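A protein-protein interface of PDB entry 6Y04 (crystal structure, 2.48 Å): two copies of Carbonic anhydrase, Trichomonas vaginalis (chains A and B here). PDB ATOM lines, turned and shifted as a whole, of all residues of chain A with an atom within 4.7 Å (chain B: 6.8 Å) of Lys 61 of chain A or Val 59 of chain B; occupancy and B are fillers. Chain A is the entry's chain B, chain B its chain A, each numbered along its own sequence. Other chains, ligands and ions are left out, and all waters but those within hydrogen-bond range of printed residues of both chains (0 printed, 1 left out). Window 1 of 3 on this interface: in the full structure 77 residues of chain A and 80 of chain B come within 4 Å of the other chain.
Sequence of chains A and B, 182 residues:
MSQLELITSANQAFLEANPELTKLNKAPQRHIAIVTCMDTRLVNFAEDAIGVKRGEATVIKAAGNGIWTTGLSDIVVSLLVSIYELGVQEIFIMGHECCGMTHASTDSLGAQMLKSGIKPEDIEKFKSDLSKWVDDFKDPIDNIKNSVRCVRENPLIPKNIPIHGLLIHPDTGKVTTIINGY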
ATOM      1  N   THR A  36      -1.125  -0.207   9.522  1.00  0.00           N
ATOM      2  CA  THR A  36      -0.993   0.922  10.428  1.00  0.00           C
ATOM      3  C   THR A  36      -2.181   0.963  11.384  1.00  0.00           C
ATOM      4  O   THR A  36      -2.989   0.040  11.403  1.00  0.00           O
ATOM      5  CB  THR A  36      -0.665   2.224   9.682  1.00  0.00           C
ATOM      6  OG1 THR A  36      -0.143   3.149  10.637  1.00  0.00           O
ATOM      7  CG2 THR A  36      -1.845   2.832   8.960  1.00  0.00           C
ATOM      8  N   CYS A  37      -2.255   2.022  12.193  1.00  0.00           N
ATOM      9  CA  CYS A  37      -3.228   2.120  13.271  1.00  0.00           C
ATOM     10  C   CYS A  37      -4.510   2.804  12.794  1.00  0.00           C
ATOM     11  O   CYS A  37      -4.512   3.527  11.802  1.00  0.00           O
ATOM     12  CB  CYS A  37      -2.646   2.884  14.452  1.00  0.00           C
ATOM     13  SG  CYS A  37      -3.754   2.858  15.882  1.00  0.00           S
ATOM     14  N   MET A  38      -5.602   2.581  13.528  1.00  0.00           N
ATOM     15  CA  MET A  38      -6.890   3.169  13.206  1.00  0.00           C
ATOM     16  C   MET A  38      -6.946   4.635  13.645  1.00  0.00           C
ATOM     17  O   MET A  38      -7.945   5.298  13.395  1.00  0.00           O
ATOM     18  CB  MET A  38      -8.025   2.404  13.903  1.00  0.00           C
ATOM     19  CG  MET A  38      -8.060   2.618  15.403  1.00  0.00           C
ATOM     20  SD  MET A  38      -9.376   1.704  16.247  1.00  0.00           S
ATOM     21  CE  MET A  38      -9.275   2.420  17.886  1.00  0.00           C
ATOM     22  N   LEU A  42      -4.248   9.794  11.836  1.00  0.00           N
ATOM     23  CA  LEU A  42      -3.526   9.265  10.685  1.00  0.00           C
ATOM     24  C   LEU A  42      -4.408   9.295   9.438  1.00  0.00           C
ATOM     25  O   LEU A  42      -3.894   9.152   8.332  1.00  0.00           O
ATOM     26  CB  LEU A  42      -3.047   7.842  10.993  1.00  0.00           C
ATOM     27  CG  LEU A  42      -2.134   7.694  12.211  1.00  0.00           C
ATOM     28  CD1 LEU A  42      -1.738   6.240  12.417  1.00  0.00           C
ATOM     29  CD2 LEU A  42      -0.892   8.563  12.090  1.00  0.00           C
ATOM     30  N   VAL A  43      -5.722   9.496   9.622  1.00  0.00           N
ATOM     31  CA  VAL A  43      -6.686   9.525   8.527  1.00  0.00           C
ATOM     32  C   VAL A  43      -6.443  10.765   7.664  1.00  0.00           C
ATOM     33  O   VAL A  43      -6.462  11.886   8.169  1.00  0.00           O
ATOM     34  CB  VAL A  43      -8.131   9.493   9.057  1.00  0.00           C
ATOM     35  CG1 VAL A  43      -9.163   9.619   7.948  1.00  0.00           C
ATOM     36  CG2 VAL A  43      -8.399   8.254   9.894  1.00  0.00           C
ATOM     37  N   GLU A  47      -0.662   8.533   4.721  1.00  0.00           N
ATOM     38  CA  GLU A  47      -0.300   8.155   3.365  1.00  0.00           C
ATOM     39  C   GLU A  47       0.462   9.295   2.706  1.00  0.00           C
ATOM     40  O   GLU A  47       1.442   9.050   2.012  1.00  0.00           O
ATOM     41  CB  GLU A  47      -1.522   7.749   2.543  1.00  0.00           C
ATOM     42  CG  GLU A  47      -2.227   6.524   3.093  1.00  0.00           C
ATOM     43  CD  GLU A  47      -3.299   6.764   4.150  1.00  0.00           C
ATOM     44  OE1 GLU A  47      -3.490   7.930   4.618  1.00  0.00           O
ATOM     45  OE2 GLU A  47      -3.964   5.767   4.502  1.00  0.00           O
ATOM     46  N   VAL A  59      -3.840  -0.796   2.261  1.00  0.00           N
ATOM     47  CA  VAL A  59      -3.683  -0.236   3.594  1.00  0.00           C
ATOM     48  C   VAL A  59      -4.596  -0.997   4.552  1.00  0.00           C
ATOM     49  O   VAL A  59      -5.806  -1.067   4.344  1.00  0.00           O
ATOM     50  CB  VAL A  59      -3.939   1.287   3.628  1.00  0.00           C
ATOM     51  CG1 VAL A  59      -3.789   1.858   5.029  1.00  0.00           C
ATOM     52  CG2 VAL A  59      -3.027   2.036   2.668  1.00  0.00           C
ATOM     53  N   ILE A  60      -3.978  -1.574   5.591  1.00  0.00           N
ATOM     54  CA  ILE A  60      -4.647  -2.403   6.578  1.00  0.00           C
ATOM     55  C   ILE A  60      -4.526  -1.660   7.902  1.00  0.00           C
ATOM     56  O   ILE A  60      -3.427  -1.256   8.252  1.00  0.00           O
ATOM     57  CB  ILE A  60      -3.961  -3.785   6.611  1.00  0.00           C
ATOM     58  CG1 ILE A  60      -4.052  -4.488   5.254  1.00  0.00           C
ATOM     59  CG2 ILE A  60      -4.512  -4.667   7.724  1.00  0.00           C
ATOM     60  CD1 ILE A  60      -2.826  -5.303   4.891  1.00  0.00           C
ATOM     61  N   LYS A  61      -5.644  -1.432   8.599  1.00  0.00           N
ATOM     62  CA  LYS A  61      -5.606  -0.648   9.826  1.00  0.00           C
ATOM     63  C   LYS A  61      -6.430  -1.295  10.939  1.00  0.00           C
ATOM     64  O   LYS A  61      -7.595  -1.662  10.731  1.00  0.00           O
ATOM     65  CB  LYS A  61      -6.214   0.740   9.623  1.00  0.00           C
ATOM     66  CG  LYS A  61      -5.528   1.675   8.647  1.00  0.00           C
ATOM     67  CD  LYS A  61      -6.101   3.056   8.855  1.00  0.00           C
ATOM     68  CE  LYS A  61      -5.662   4.079   7.841  1.00  0.00           C
ATOM     69  NZ  LYS A  61      -6.310   5.380   8.116  1.00  0.00           N
ATOM     70  N   ALA A  62      -5.823  -1.355  12.135  1.00  0.00           N
ATOM     71  CA  ALA A  62      -6.476  -1.807  13.354  1.00  0.00           C
ATOM     72  C   ALA A  62      -5.821  -1.110  14.539  1.00  0.00           C
ATOM     73  O   ALA A  62      -4.695  -0.633  14.429  1.00  0.00           O
ATOM     74  CB  ALA A  62      -6.372  -3.313  13.497  1.00  0.00           C
ATOM     75  N   ILE B  32     -17.336   8.599  15.532  1.00  0.00           N
ATOM     76  CA  ILE B  32     -17.739   7.567  14.589  1.00  0.00           C
ATOM     77  C   ILE B  32     -16.541   6.692  14.220  1.00  0.00           C
ATOM     78  O   ILE B  32     -15.400   7.151  14.175  1.00  0.00           O
ATOM     79  CB  ILE B  32     -18.436   8.169  13.350  1.00  0.00           C
ATOM     80  CG1 ILE B  32     -17.517   9.116  12.572  1.00  0.00           C
ATOM     81  CG2 ILE B  32     -19.748   8.838  13.740  1.00  0.00           C
ATOM     82  CD1 ILE B  32     -18.102   9.607  11.265  1.00  0.00           C
ATOM     83  N   ALA B  33     -16.828   5.411  13.986  1.00  0.00           N
ATOM     84  CA  ALA B  33     -15.854   4.466  13.475  1.00  0.00           C
ATOM     85  C   ALA B  33     -16.292   4.013  12.083  1.00  0.00           C
ATOM     86  O   ALA B  33     -17.462   3.677  11.883  1.00  0.00           O
ATOM     87  CB  ALA B  33     -15.744   3.293  14.424  1.00  0.00           C
ATOM     88  N   ILE B  34     -15.343   4.005  11.134  1.00  0.00           N
ATOM     89  CA  ILE B  34     -15.550   3.452   9.802  1.00  0.00           C
ATOM     90  C   ILE B  34     -14.780   2.137   9.689  1.00  0.00           C
ATOM     91  O   ILE B  34     -13.583   2.107   9.971  1.00  0.00           O
ATOM     92  CB  ILE B  34     -15.105   4.435   8.700  1.00  0.00           C
ATOM     93  CG1 ILE B  34     -15.565   5.877   8.949  1.00  0.00           C
ATOM     94  CG2 ILE B  34     -15.500   3.931   7.318  1.00  0.00           C
ATOM     95  CD1 ILE B  34     -17.068   6.105   8.890  1.00  0.00           C
ATOM     96  N   VAL B  35     -15.473   1.071   9.255  1.00  0.00           N
ATOM     97  CA  VAL B  35     -14.830  -0.181   8.872  1.00  0.00           C
ATOM     98  C   VAL B  35     -14.934  -0.347   7.359  1.00  0.00           C
ATOM     99  O   VAL B  35     -16.033  -0.396   6.813  1.00  0.00           O
ATOM    100  CB  VAL B  35     -15.411  -1.401   9.625  1.00  0.00           C
ATOM    101  CG1 VAL B  35     -14.733  -2.702   9.210  1.00  0.00           C
ATOM    102  CG2 VAL B  35     -15.342  -1.224  11.140  1.00  0.00           C
ATOM    103  N   THR B  36     -13.789  -0.432   6.681  1.00  0.00           N
ATOM    104  CA  THR B  36     -13.822  -0.550   5.232  1.00  0.00           C
ATOM    105  C   THR B  36     -12.726  -1.504   4.760  1.00  0.00           C
ATOM    106  O   THR B  36     -12.063  -2.143   5.576  1.00  0.00           O
ATOM    107  CB  THR B  36     -13.885   0.826   4.551  1.00  0.00           C
ATOM    108  OG1 THR B  36     -14.363   0.626   3.221  1.00  0.00           O
ATOM    109  CG2 THR B  36     -12.561   1.563   4.536  1.00  0.00           C
ATOM    110  N   MET B  38      -9.309  -2.882   2.475  1.00  0.00           N
ATOM    111  CA  MET B  38      -7.929  -2.461   2.295  1.00  0.00           C
ATOM    112  C   MET B  38      -7.679  -2.035   0.846  1.00  0.00           C
ATOM    113  O   MET B  38      -6.573  -1.614   0.521  1.00  0.00           O
ATOM    114  CB  MET B  38      -6.972  -3.601   2.657  1.00  0.00           C
ATOM    115  CG  MET B  38      -7.004  -4.730   1.654  1.00  0.00           C
ATOM    116  SD  MET B  38      -5.879  -6.072   2.058  1.00  0.00           S
ATOM    117  CE  MET B  38      -5.955  -7.034   0.546  1.00  0.00           C
ATOM    118  N   GLU B  47     -12.655   8.360   2.398  1.00  0.00           N
ATOM    119  CA  GLU B  47     -12.946   9.319   3.450  1.00  0.00           C
ATOM    120  C   GLU B  47     -13.514  10.594   2.838  1.00  0.00           C
ATOM    121  O   GLU B  47     -14.477  11.158   3.367  1.00  0.00           O
ATOM    122  CB  GLU B  47     -11.693   9.638   4.269  1.00  0.00           C
ATOM    123  CG  GLU B  47     -11.158   8.451   5.047  1.00  0.00           C
ATOM    124  CD  GLU B  47     -10.198   7.520   4.315  1.00  0.00           C
ATOM    125  OE1 GLU B  47      -9.898   7.762   3.107  1.00  0.00           O
ATOM    126  OE2 GLU B  47      -9.742   6.548   4.963  1.00  0.00           O
ATOM    127  N   VAL B  52     -15.513  12.592   5.451  1.00  0.00           N
ATOM    128  CA  VAL B  52     -14.873  12.396   6.734  1.00  0.00           C
ATOM    129  C   VAL B  52     -13.475  12.989   6.630  1.00  0.00           C
ATOM    130  O   VAL B  52     -12.746  12.694   5.682  1.00  0.00           O
ATOM    131  CB  VAL B  52     -14.876  10.909   7.132  1.00  0.00           C
ATOM    132  CG1 VAL B  52     -13.753  10.557   8.094  1.00  0.00           C
ATOM    133  CG2 VAL B  52     -16.227  10.498   7.687  1.00  0.00           C
ATOM    134  N   ALA B  57     -12.874  10.584  12.726  1.00  0.00           N
ATOM    135  CA  ALA B  57     -13.293   9.195  12.857  1.00  0.00           C
ATOM    136  C   ALA B  57     -12.079   8.293  13.053  1.00  0.00           C
ATOM    137  O   ALA B  57     -10.974   8.641  12.660  1.00  0.00           O
ATOM    138  CB  ALA B  57     -14.060   8.770  11.629  1.00  0.00           C
ATOM    139  N   THR B  58     -12.297   7.117  13.647  1.00  0.00           N
ATOM    140  CA  THR B  58     -11.351   6.024  13.493  1.00  0.00           C
ATOM    141  C   THR B  58     -11.718   5.268  12.220  1.00  0.00           C
ATOM    142  O   THR B  58     -12.900   5.145  11.886  1.00  0.00           O
ATOM    143  CB  THR B  58     -11.330   5.102  14.722  1.00  0.00           C
ATOM    144  OG1 THR B  58     -12.667   4.678  14.981  1.00  0.00           O
ATOM    145  CG2 THR B  58     -10.754   5.767  15.952  1.00  0.00           C
ATOM    146  N   VAL B  59     -10.687   4.779  11.518  1.00  0.00           N
ATOM    147  CA  VAL B  59     -10.868   4.004  10.304  1.00  0.00           C
ATOM    148  C   VAL B  59     -10.147   2.670  10.471  1.00  0.00           C
ATOM    149  O   VAL B  59      -8.957   2.639  10.764  1.00  0.00           O
ATOM    150  CB  VAL B  59     -10.385   4.771   9.052  1.00  0.00           C
ATOM    151  CG1 VAL B  59     -10.563   3.951   7.779  1.00  0.00           C
ATOM    152  CG2 VAL B  59     -11.062   6.133   8.921  1.00  0.00           C
ATOM    153  N   ILE B  60     -10.900   1.578  10.286  1.00  0.00           N
ATOM    154  CA  ILE B  60     -10.437   0.210  10.460  1.00  0.00           C
ATOM    155  C   ILE B  60     -10.545  -0.441   9.086  1.00  0.00           C
ATOM    156  O   ILE B  60     -11.588  -0.326   8.456  1.00  0.00           O
ATOM    157  CB  ILE B  60     -11.333  -0.495  11.506  1.00  0.00           C
ATOM    158  CG1 ILE B  60     -11.284   0.227  12.857  1.00  0.00           C
ATOM    159  CG2 ILE B  60     -11.003  -1.976  11.637  1.00  0.00           C
ATOM    160  CD1 ILE B  60     -12.587   0.232  13.625  1.00  0.00           C
ATOM    161  N   LYS B  61      -9.468  -1.074   8.606  1.00  0.00           N
ATOM    162  CA  LYS B  61      -9.479  -1.653   7.271  1.00  0.00           C
ATOM    163  C   LYS B  61      -8.884  -3.059   7.264  1.00  0.00           C
ATOM    164  O   LYS B  61      -7.787  -3.283   7.767  1.00  0.00           O
ATOM    165  CB  LYS B  61      -8.649  -0.825   6.287  1.00  0.00           C
ATOM    166  CG  LYS B  61      -9.097   0.605   6.016  1.00  0.00           C
ATOM    167  CD  LYS B  61      -8.379   1.125   4.796  1.00  0.00           C
ATOM    168  CE  LYS B  61      -8.515   2.609   4.576  1.00  0.00           C
ATOM    169  NZ  LYS B  61      -7.688   3.015   3.416  1.00  0.00           N
ATOM    170  N   ALA B  62      -9.598  -3.984   6.615  1.00  0.00           N
ATOM    171  CA  ALA B  62      -9.123  -5.328   6.338  1.00  0.00           C
ATOM    172  C   ALA B  62      -9.686  -5.773   4.993  1.00  0.00           C
ATOM    173  O   ALA B  62     -10.697  -5.242   4.544  1.00  0.00           O
ATOM    174  CB  ALA B  62      -9.550  -6.270   7.442  1.00  0.00           C
ATOM    175  N   ASP B  74      -9.262  -8.708  15.106  1.00  0.00           N
ATOM    176  CA  ASP B  74      -8.611  -7.414  14.949  1.00  0.00           C
ATOM    177  C   ASP B  74      -9.674  -6.317  14.829  1.00  0.00           C
ATOM    178  O   ASP B  74      -9.591  -5.289  15.505  1.00  0.00           O
ATOM    179  CB  ASP B  74      -7.679  -7.381  13.727  1.00  0.00           C
ATOM    180  CG  ASP B  74      -6.444  -8.268  13.798  1.00  0.00           C
ATOM    181  OD1 ASP B  74      -5.977  -8.552  14.910  1.00  0.00           O
ATOM    182  OD2 ASP B  74      -5.958  -8.674  12.734  1.00  0.00           O
ATOM    183  N   ILE B  75     -10.681  -6.551  13.972  1.00  0.00           N
ATOM    184  CA  ILE B  75     -11.676  -5.536  13.662  1.00  0.00           C
ATOM    185  C   ILE B  75     -12.530  -5.277  14.899  1.00  0.00           C
ATOM    186  O   ILE B  75     -12.734  -4.127  15.285  1.00  0.00           O
ATOM    187  CB  ILE B  75     -12.509  -5.892  12.413  1.00  0.00           C
ATOM    188  CG1 ILE B  75     -11.663  -5.793  11.143  1.00  0.00           C
ATOM    189  CG2 ILE B  75     -13.734  -4.997  12.313  1.00  0.00           C
ATOM    190  CD1 ILE B  75     -12.430  -6.088   9.867  1.00  0.00           C
ATOM    191  N   SER B  78     -10.763  -3.356  17.618  1.00  0.00           N
ATOM    192  CA  SER B  78     -10.683  -1.976  17.166  1.00  0.00           C
ATOM    193  C   SER B  78     -11.966  -1.221  17.499  1.00  0.00           C
ATOM    194  O   SER B  78     -11.913  -0.065  17.906  1.00  0.00           O
ATOM    195  CB  SER B  78     -10.377  -1.907  15.692  1.00  0.00           C
ATOM    196  OG  SER B  78      -9.092  -2.452  15.420  1.00  0.00           O
ATOM    197  N   SER B  82     -12.508   1.792  20.099  1.00  0.00           N
ATOM    198  CA  SER B  82     -13.139   2.998  19.590  1.00  0.00           C
ATOM    199  C   SER B  82     -14.240   3.459  20.543  1.00  0.00           C
ATOM    200  O   SER B  82     -14.309   4.640  20.889  1.00  0.00           O
ATOM    201  CB  SER B  82     -13.674   2.794  18.193  1.00  0.00           C
ATOM    202  OG  SER B  82     -12.611   2.641  17.267  1.00  0.00           O
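CA of Thr 58 of chain B touches O of Met 38 of chain A, at 3.5 Å.
Val 43 of chain A touches Glu 47 of chain B.
Val 43 of chain A touches Ala 57 of chain B (CG2 to O, 3.8 Å).
CG2 of Val 43 of chain A touches CG2 of Val 59 of chain B, at 3.5 Å.
O of Val 59 of chain A touches CD of Lys 61 of chain B, at 3.4 Å.
Lys 61 of chain B touches Ile 60 of chain A.
Val 59 of chain B touches Lys 61 of chain A.
Lys 61 of chain A touches Ile 60 of chain B (O to CA, 3.4 Å).
OG of Ser 78 of chain B touches CA of Ala 62 of chain A (3.4 Å).
The backbone NH (N) of Val 59 of chain B sits at hydrogen-bond distance from the backbone carbonyl oxygen (O) of Met 38 of chain A (3.4 Å).
The side-chain sulfur of Met 38 of chain A sits close to the backbone carbonyl oxygen of Ser 78 of chain B (3.5 Å).
The backbone NH (N) of Lys 61 of chain B is in hydrogen-bond range of the backbone carbonyl oxygen (O) of Lys 61 of chain A (2.9 Å).
The side-chain hydroxyl (OG) of Ser 82 of chain B sits close to the side-chain sulfur (SD) of Met 38 of chain A, at 3.5 Å.
O of Met 38 of chain B lies within hydrogen-bond range of N of Val 59 of chain A (3.3 Å).
The backbone carbonyl oxygen of Glu 47 of chain B lies within hydrogen-bond range of the backbone NH of Val 52 of chain B (2.7 Å).
N of Met 38 of chain B is in hydrogen-bond range of O of Ala 62 of chain B (3.4 Å).
The backbone carbonyl oxygen (O) of Ser 78 of chain B sits at hydrogen-bond distance from the side-chain hydroxyl (OG) of Ser 82 of chain B (2.9 Å).
The backbone NH (N) of Ile 34 of chain B sits at hydrogen-bond distance from the backbone carbonyl oxygen (O) of Thr 58 of chain B (2.8 Å).
The side-chain hydroxyl (OG1) of Thr 58 of chain B lies within hydrogen-bond range of the side-chain hydroxyl (OG) of Ser 82 of chain B (3.1 Å).
The backbone carbonyl oxygen of Ile 34 of chain B is in hydrogen-bond range of the backbone NH of Ile 60 of chain B, at 2.8 Å.
Thr 36 of chain A touches none of the printed residues of chain B.
Of the printed residues of chain B, Met 38 of chain A touches Thr 58 (3.5 Å), Val 59 (3.2 Å), Ser 78 (3.5 Å) and Ser 82 (3.4 Å).
Printed residues of chain B within 4 Å of Val 59 of chain A: Met 38 (3.3 Å) and Lys 61 (3.4 Å).
Of chain B, only Val 59, Ile 60 and Lys 61 come within 4 Å of Lys 61 of chain A.
Thr 36 of chain B touches none of the printed residues of chain A.
Of the printed residues of chain A, Ala 57 of chain B touches Val 43 (3.8 Å).
Of the printed residues of chain A, Thr 58 of chain B touches Met 38 (3.5 Å).
Printed residues of chain A within 4 Å of Val 59 of chain B: Met 38 (3.2 Å), Val 43 (3.5 Å) and Lys 61 (3.5 Å).
Printed residues of chain A within 4 Å of Lys 61 of chain B: Val 59, Ile 60 and Lys 61.
The nearest residue of chain B that does not touch Lys 61 of chain A is Glu 47 of chain B (4.8 Å).
The nearest printed residue of chain B that does not touch Met 38 of chain A is Ile 60 of chain B (4.1 Å).
Met 38 of chain A touches Val 59 of chain B, and with the chains exchanged Val 59 of chain A touches Met 38 of chain B.
Val 59 of chain A touches Lys 61 of chain B, and with the chains exchanged Lys 61 of chain A touches Val 59 of chain B.
Ile 60 of chain A touches Lys 61 of chain B, and with the chains exchanged Lys 61 of chain A touches Ile 60 of chain B.
Lys 61 of chain B touches its own counterpart, Lys 61 of chain A.
Positions printed for both chains: 36, 38, 47, 59, 60, 61 and 62.
Of the 14 pairs that touch across the chains among the printed residues, 7 have their exchanged pair printed and touching as well.
Of the 18 printed residues of chain B, 9 touch a printed residue of chain A.
Hydrophobic or aromatic side chains of chain B within 4 Å of the printed part of chain A: Met 38, Val 59 and Ile 60.
Of the 10 printed residues of chain A, 6 touch a printed residue of chain B.
Along chain A the printed residues that touch a printed residue of chain B span positions 38 to 62.
Among the printed residues, no Asp or Glu carboxylate lies within 4 Å of a Lys or Arg side-chain nitrogen of the other chain.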
